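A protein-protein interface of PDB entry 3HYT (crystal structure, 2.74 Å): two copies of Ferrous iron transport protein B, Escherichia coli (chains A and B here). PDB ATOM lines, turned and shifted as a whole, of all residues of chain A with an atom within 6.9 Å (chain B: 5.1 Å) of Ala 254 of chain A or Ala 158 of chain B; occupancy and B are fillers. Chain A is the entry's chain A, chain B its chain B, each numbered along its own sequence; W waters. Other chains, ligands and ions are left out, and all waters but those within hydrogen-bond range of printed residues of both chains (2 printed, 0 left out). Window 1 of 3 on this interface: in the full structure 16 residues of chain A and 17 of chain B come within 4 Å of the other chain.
O of Glu 157 of chain B sits at hydrogen-bond distance from NE2 of Gln 250 of chain A.
NE2 of Gln 250 of chain A sits close to N of Leu 161 of chain B (3.3 Å).
The backbone NH (N) of Gly 155 of chain B sits at hydrogen-bond distance from the side-chain carboxylate (OD1) of Asp 257 of chain A, at 3.1 Å.
O of Arg 154 of chain B lies close to OD1 of Asp 257 of chain A, at 3.4 Å.
Water W1 lies within hydrogen-bond range of NH1 of Arg 154 of chain B and O of Cys 256 of chain A.
Water W2 lies within hydrogen-bond range of NE2 of Gln 250 of chain A (3.0 Å) and O of Lys 160 of chain B (3.2 Å).
CD2 of Tyr 249 of chain A touches OE1 of Glu 157 of chain B, 3.96 Å away.
CB of Lys 160 of chain B touches NE2 of Gln 250 of chain A, 3.7 Å away.
Ala 253 of chain A touches Arg 154 of chain B (O to CG, 3.7 Å).
CB of Ala 253 of chain A touches CG of Glu 157 of chain B, 3.7 Å away.
Ala 158 of chain B touches Ala 254 of chain A.
Leu 161 of chain B touches Ala 254 of chain A.
Cys 256 of chain A touches Arg 154 of chain B.
CG2 of Ile 146 of chain B touches OD2 of Asp 257 of chain A, 3.9 Å away.
Ala 158 of chain B touches Asp 257 of chain A (CB to OD2, 3.6 Å).
Printed residues of chain B within 4 Å of Gln 250 of chain A: Glu 157, Lys 160 and Leu 161.
Of the printed residues of chain B, Ala 254 of chain A touches Ala 158 and Leu 161.
Val 259 of chain A touches none of the printed residues of chain B.
Of the printed residues of chain A, Glu 157 of chain B touches Tyr 249, Gln 250 and Ala 253.
The nearest printed residue of chain B that does not touch Ala 254 of chain A is Arg 154 of chain B (4.8 Å).
The nearest residue of chain A that does not touch Ala 158 of chain B is Val 258 of chain A (5.1 Å).
The nearest printed residue of chain B that does not touch Tyr 249 of chain A is Gly 153 of chain B (4.9 Å).
No position is printed for both chains.
Hydrophobic or aromatic side chains of chain B within 4 Å of the printed part of chain A: Ile 146, Ala 158 and Leu 161.
Printed residues of chain A that touch a printed residue of chain B: Tyr 249, Gln 250, Ala 253, Ala 254, Cys 256 and Asp 257.
Among the printed residues, no Asp or Glu carboxylate lies within 4 Å of a Lys or Arg side-chain nitrogen of the other chain.
The backbone carbonyl oxygen (O) of Ile 252 of chain A is in hydrogen-bond range of the side-chain sulfur (SG) of Cys 256 of chain A, 3.4 Å away.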
ATOM      1  N   ARG A 140     -12.953  19.512 -16.689  1.00  0.00           N
ATOM      2  CA  ARG A 140     -12.281  18.483 -17.477  1.00  0.00           C
ATOM      3  C   ARG A 140     -13.077  18.071 -18.713  1.00  0.00           C
ATOM      4  O   ARG A 140     -12.494  17.751 -19.748  1.00  0.00           O
ATOM      5  CB  ARG A 140     -11.965  17.275 -16.601  1.00  0.00           C
ATOM      6  CG  ARG A 140     -10.793  17.513 -15.679  1.00  0.00           C
ATOM      7  CD  ARG A 140     -10.898  16.707 -14.403  1.00  0.00           C
ATOM      8  NE  ARG A 140      -9.758  16.968 -13.523  1.00  0.00           N
ATOM      9  CZ  ARG A 140      -9.673  17.989 -12.670  1.00  0.00           C
ATOM     10  NH1 ARG A 140     -10.663  18.868 -12.555  1.00  0.00           N
ATOM     11  NH2 ARG A 140      -8.588  18.128 -11.924  1.00  0.00           N
ATOM     12  N   TYR A 249      -9.627   4.950 -21.859  1.00  0.00           N
ATOM     13  CA  TYR A 249      -9.892   4.526 -20.489  1.00  0.00           C
ATOM     14  C   TYR A 249      -9.161   5.412 -19.475  1.00  0.00           C
ATOM     15  O   TYR A 249      -9.716   5.755 -18.424  1.00  0.00           O
ATOM     16  CB  TYR A 249      -9.550   3.050 -20.251  1.00  0.00           C
ATOM     17  CG  TYR A 249      -9.742   2.672 -18.801  1.00  0.00           C
ATOM     18  CD1 TYR A 249     -11.022   2.509 -18.263  1.00  0.00           C
ATOM     19  CD2 TYR A 249      -8.653   2.537 -17.949  1.00  0.00           C
ATOM     20  CE1 TYR A 249     -11.207   2.194 -16.923  1.00  0.00           C
ATOM     21  CE2 TYR A 249      -8.830   2.226 -16.606  1.00  0.00           C
ATOM     22  CZ  TYR A 249     -10.105   2.054 -16.104  1.00  0.00           C
ATOM     23  OH  TYR A 249     -10.263   1.739 -14.776  1.00  0.00           O
ATOM     24  N   GLN A 250      -7.923   5.778 -19.802  1.00  0.00           N
ATOM     25  CA  GLN A 250      -7.110   6.641 -18.960  1.00  0.00           C
ATOM     26  C   GLN A 250      -7.803   7.984 -18.704  1.00  0.00           C
ATOM     27  O   GLN A 250      -7.695   8.548 -17.613  1.00  0.00           O
ATOM     28  CB  GLN A 250      -5.730   6.860 -19.587  1.00  0.00           C
ATOM     29  CG  GLN A 250      -4.688   7.404 -18.610  1.00  0.00           C
ATOM     30  CD  GLN A 250      -3.530   8.103 -19.290  1.00  0.00           C
ATOM     31  OE1 GLN A 250      -3.628   8.536 -20.436  1.00  0.00           O
ATOM     32  NE2 GLN A 250      -2.420   8.229 -18.574  1.00  0.00           N
ATOM     33  N   CYS A 251      -8.513   8.479 -19.716  1.00  0.00           N
ATOM     34  CA  CYS A 251      -9.250   9.734 -19.615  1.00  0.00           C
ATOM     35  C   CYS A 251     -10.430   9.598 -18.669  1.00  0.00           C
ATOM     36  O   CYS A 251     -10.626  10.443 -17.791  1.00  0.00           O
ATOM     37  CB  CYS A 251      -9.734  10.182 -20.998  1.00  0.00           C
ATOM     38  SG  CYS A 251     -10.648  11.737 -21.001  1.00  0.00           S
ATOM     39  N   ILE A 252     -11.214   8.538 -18.857  1.00  0.00           N
ATOM     40  CA  ILE A 252     -12.358   8.242 -17.992  1.00  0.00           C
ATOM     41  C   ILE A 252     -11.900   8.051 -16.542  1.00  0.00           C
ATOM     42  O   ILE A 252     -12.428   8.688 -15.628  1.00  0.00           O
ATOM     43  CB  ILE A 252     -13.135   6.977 -18.473  1.00  0.00           C
ATOM     44  CG1 ILE A 252     -13.585   7.111 -19.937  1.00  0.00           C
ATOM     45  CG2 ILE A 252     -14.312   6.662 -17.544  1.00  0.00           C
ATOM     46  CD1 ILE A 252     -14.431   8.337 -20.239  1.00  0.00           C
ATOM     47  N   ALA A 253     -10.907   7.188 -16.351  1.00  0.00           N
ATOM     48  CA  ALA A 253     -10.410   6.858 -15.021  1.00  0.00           C
ATOM     49  C   ALA A 253      -9.825   8.065 -14.293  1.00  0.00           C
ATOM     50  O   ALA A 253     -10.065   8.242 -13.100  1.00  0.00           O
ATOM     51  CB  ALA A 253      -9.398   5.724 -15.092  1.00  0.00           C
ATOM     52  N   ALA A 254      -9.079   8.899 -15.013  1.00  0.00           N
ATOM     53  CA  ALA A 254      -8.455  10.079 -14.421  1.00  0.00           C
ATOM     54  C   ALA A 254      -9.498  11.087 -13.954  1.00  0.00           C
ATOM     55  O   ALA A 254      -9.310  11.757 -12.937  1.00  0.00           O
ATOM     56  CB  ALA A 254      -7.495  10.720 -15.389  1.00  0.00           C
ATOM     57  N   ILE A 255     -10.593  11.186 -14.703  1.00  0.00           N
ATOM     58  CA  ILE A 255     -11.720  12.030 -14.324  1.00  0.00           C
ATOM     59  C   ILE A 255     -12.355  11.523 -13.021  1.00  0.00           C
ATOM     60  O   ILE A 255     -12.402  12.256 -12.035  1.00  0.00           O
ATOM     61  CB  ILE A 255     -12.756  12.145 -15.472  1.00  0.00           C
ATOM     62  CG1 ILE A 255     -12.267  13.144 -16.529  1.00  0.00           C
ATOM     63  CG2 ILE A 255     -14.116  12.581 -14.944  1.00  0.00           C
ATOM     64  CD1 ILE A 255     -12.943  13.000 -17.890  1.00  0.00           C
ATOM     65  N   CYS A 256     -12.804  10.267 -13.022  1.00  0.00           N
ATOM     66  CA  CYS A 256     -13.390   9.619 -11.842  1.00  0.00           C
ATOM     67  C   CYS A 256     -12.495   9.708 -10.612  1.00  0.00           C
ATOM     68  O   CYS A 256     -12.983   9.867  -9.494  1.00  0.00           O
ATOM     69  CB  CYS A 256     -13.680   8.145 -12.134  1.00  0.00           C
ATOM     70  SG  CYS A 256     -14.877   7.860 -13.448  1.00  0.00           S
ATOM     71  N   ASP A 257     -11.187   9.597 -10.834  1.00  0.00           N
ATOM     72  CA  ASP A 257     -10.191   9.655  -9.769  1.00  0.00           C
ATOM     73  C   ASP A 257     -10.213  10.987  -9.024  1.00  0.00           C
ATOM     74  O   ASP A 257     -10.119  11.013  -7.798  1.00  0.00           O
ATOM     75  CB  ASP A 257      -8.794   9.414 -10.342  1.00  0.00           C
ATOM     76  CG  ASP A 257      -7.725   9.365  -9.271  1.00  0.00           C
ATOM     77  OD1 ASP A 257      -7.551   8.297  -8.649  1.00  0.00           O
ATOM     78  OD2 ASP A 257      -7.048  10.393  -9.058  1.00  0.00           O
ATOM     79  N   VAL A 258     -10.331  12.082  -9.771  1.00  0.00           N
ATOM     80  CA  VAL A 258     -10.306  13.424  -9.197  1.00  0.00           C
ATOM     81  C   VAL A 258     -11.701  13.843  -8.759  1.00  0.00           C
ATOM     82  O   VAL A 258     -11.884  14.425  -7.694  1.00  0.00           O
ATOM     83  CB  VAL A 258      -9.755  14.473 -10.212  1.00  0.00           C
ATOM     84  CG1 VAL A 258      -9.814  15.883  -9.628  1.00  0.00           C
ATOM     85  CG2 VAL A 258      -8.336  14.131 -10.638  1.00  0.00           C
ATOM     86  N   VAL A 259     -12.679  13.515  -9.591  1.00  0.00           N
ATOM     87  CA  VAL A 259     -14.039  14.033  -9.481  1.00  0.00           C
ATOM     88  C   VAL A 259     -14.925  13.290  -8.465  1.00  0.00           C
ATOM     89  O   VAL A 259     -15.766  13.908  -7.806  1.00  0.00           O
ATOM     90  CB  VAL A 259     -14.676  14.083 -10.902  1.00  0.00           C
ATOM     91  CG1 VAL A 259     -16.192  14.002 -10.873  1.00  0.00           C
ATOM     92  CG2 VAL A 259     -14.198  15.320 -11.631  1.00  0.00           C
ATOM     93  N   ILE B 146      -3.677  15.003  -7.289  1.00  0.00           N
ATOM     94  CA  ILE B 146      -4.077  13.693  -7.803  1.00  0.00           C
ATOM     95  C   ILE B 146      -4.296  12.693  -6.661  1.00  0.00           C
ATOM     96  O   ILE B 146      -3.343  12.285  -6.002  1.00  0.00           O
ATOM     97  CB  ILE B 146      -3.008  13.127  -8.789  1.00  0.00           C
ATOM     98  CG1 ILE B 146      -2.752  14.087  -9.970  1.00  0.00           C
ATOM     99  CG2 ILE B 146      -3.369  11.706  -9.251  1.00  0.00           C
ATOM    100  CD1 ILE B 146      -3.970  14.416 -10.840  1.00  0.00           C
ATOM    101  N   GLY B 153      -7.298   0.967 -10.990  1.00  0.00           N
ATOM    102  CA  GLY B 153      -6.066   1.650 -11.381  1.00  0.00           C
ATOM    103  C   GLY B 153      -6.237   3.133 -11.657  1.00  0.00           C
ATOM    104  O   GLY B 153      -5.529   3.695 -12.494  1.00  0.00           O
ATOM    105  N   ARG B 154      -7.167   3.766 -10.945  1.00  0.00           N
ATOM    106  CA  ARG B 154      -7.503   5.172 -11.170  1.00  0.00           C
ATOM    107  C   ARG B 154      -6.394   6.149 -10.781  1.00  0.00           C
ATOM    108  O   ARG B 154      -6.128   7.107 -11.511  1.00  0.00           O
ATOM    109  CB  ARG B 154      -8.807   5.532 -10.459  1.00  0.00           C
ATOM    110  CG  ARG B 154     -10.035   5.063 -11.197  1.00  0.00           C
ATOM    111  CD  ARG B 154     -11.264   5.155 -10.333  1.00  0.00           C
ATOM    112  NE  ARG B 154     -12.442   4.694 -11.062  1.00  0.00           N
ATOM    113  CZ  ARG B 154     -13.695   4.824 -10.641  1.00  0.00           C
ATOM    114  NH1 ARG B 154     -13.954   5.412  -9.482  1.00  0.00           N
ATOM    115  NH2 ARG B 154     -14.689   4.370 -11.391  1.00  0.00           N
ATOM    116  N   GLY B 155      -5.761   5.902  -9.634  1.00  0.00           N
ATOM    117  CA  GLY B 155      -4.650   6.727  -9.148  1.00  0.00           C
ATOM    118  C   GLY B 155      -3.486   6.780 -10.121  1.00  0.00           C
ATOM    119  O   GLY B 155      -3.153   7.846 -10.631  1.00  0.00           O
ATOM    120  N   ILE B 156      -2.880   5.621 -10.374  1.00  0.00           N
ATOM    121  CA  ILE B 156      -1.784   5.477 -11.341  1.00  0.00           C
ATOM    122  C   ILE B 156      -2.164   6.071 -12.701  1.00  0.00           C
ATOM    123  O   ILE B 156      -1.388   6.811 -13.309  1.00  0.00           O
ATOM    124  CB  ILE B 156      -1.370   3.979 -11.503  1.00  0.00           C
ATOM    125  CG1 ILE B 156      -0.877   3.399 -10.169  1.00  0.00           C
ATOM    126  CG2 ILE B 156      -0.331   3.790 -12.619  1.00  0.00           C
ATOM    127  CD1 ILE B 156       0.313   4.132  -9.537  1.00  0.00           C
ATOM    128  N   GLU B 157      -3.370   5.748 -13.152  1.00  0.00           N
ATOM    129  CA  GLU B 157      -3.922   6.271 -14.392  1.00  0.00           C
ATOM    130  C   GLU B 157      -3.849   7.794 -14.445  1.00  0.00           C
ATOM    131  O   GLU B 157      -3.344   8.360 -15.411  1.00  0.00           O
ATOM    132  CB  GLU B 157      -5.378   5.823 -14.522  1.00  0.00           C
ATOM    133  CG  GLU B 157      -5.793   5.428 -15.918  1.00  0.00           C
ATOM    134  CD  GLU B 157      -5.131   4.150 -16.398  1.00  0.00           C
ATOM    135  OE1 GLU B 157      -4.980   3.987 -17.627  1.00  0.00           O
ATOM    136  OE2 GLU B 157      -4.762   3.311 -15.548  1.00  0.00           O
ATOM    137  N   ALA B 158      -4.352   8.442 -13.395  1.00  0.00           N
ATOM    138  CA  ALA B 158      -4.414   9.904 -13.318  1.00  0.00           C
ATOM    139  C   ALA B 158      -3.036  10.537 -13.155  1.00  0.00           C
ATOM    140  O   ALA B 158      -2.781  11.621 -13.672  1.00  0.00           O
ATOM    141  CB  ALA B 158      -5.333  10.336 -12.190  1.00  0.00           C
ATOM    142  N   LEU B 159      -2.159   9.845 -12.433  1.00  0.00           N
ATOM    143  CA  LEU B 159      -0.806  10.302 -12.174  1.00  0.00           C
ATOM    144  C   LEU B 159      -0.023  10.354 -13.480  1.00  0.00           C
ATOM    145  O   LEU B 159       0.653  11.349 -13.770  1.00  0.00           O
ATOM    146  CB  LEU B 159      -0.122   9.342 -11.203  1.00  0.00           C
ATOM    147  CG  LEU B 159       0.677   9.858 -10.004  1.00  0.00           C
ATOM    148  CD1 LEU B 159       1.518   8.714  -9.474  1.00  0.00           C
ATOM    149  CD2 LEU B 159       1.562  11.065 -10.323  1.00  0.00           C
ATOM    150  N   LYS B 160      -0.129   9.279 -14.264  1.00  0.00           N
ATOM    151  CA  LYS B 160       0.547   9.158 -15.556  1.00  0.00           C
ATOM    152  C   LYS B 160       0.107  10.233 -16.548  1.00  0.00           C
ATOM    153  O   LYS B 160       0.940  10.803 -17.258  1.00  0.00           O
ATOM    154  CB  LYS B 160       0.317   7.770 -16.152  1.00  0.00           C
ATOM    155  CG  LYS B 160       1.168   6.683 -15.517  1.00  0.00           C
ATOM    156  CD  LYS B 160       1.089   5.396 -16.316  1.00  0.00           C
ATOM    157  CE  LYS B 160       2.161   4.419 -15.871  1.00  0.00           C
ATOM    158  NZ  LYS B 160       2.058   3.109 -16.581  1.00  0.00           N
ATOM    159  N   LEU B 161      -1.197  10.505 -16.589  1.00  0.00           N
ATOM    160  CA  LEU B 161      -1.743  11.581 -17.411  1.00  0.00           C
ATOM    161  C   LEU B 161      -1.152  12.938 -17.017  1.00  0.00           C
ATOM    162  O   LEU B 161      -0.736  13.712 -17.874  1.00  0.00           O
ATOM    163  CB  LEU B 161      -3.272  11.611 -17.316  1.00  0.00           C
ATOM    164  CG  LEU B 161      -4.032  12.547 -18.262  1.00  0.00           C
ATOM    165  CD1 LEU B 161      -3.777  12.188 -19.725  1.00  0.00           C
ATOM    166  CD2 LEU B 161      -5.523  12.544 -17.957  1.00  0.00           C
ATOM    167  N   ALA B 162      -1.096  13.201 -15.715  1.00  0.00           N
ATOM    168  CA  ALA B 162      -0.543  14.450 -15.200  1.00  0.00           C
ATOM    169  C   ALA B 162       0.942  14.613 -15.537  1.00  0.00           C
ATOM    170  O   ALA B 162       1.404  15.733 -15.757  1.00  0.00           O
ATOM    171  CB  ALA B 162      -0.772  14.558 -13.702  1.00  0.00           C
HETATM  172  O   HOH W   1     -12.697   7.304  -7.891  1.00  0.00           O
HETATM  173  O   HOH W   2       0.294   8.714 -19.628  1.00  0.00           O
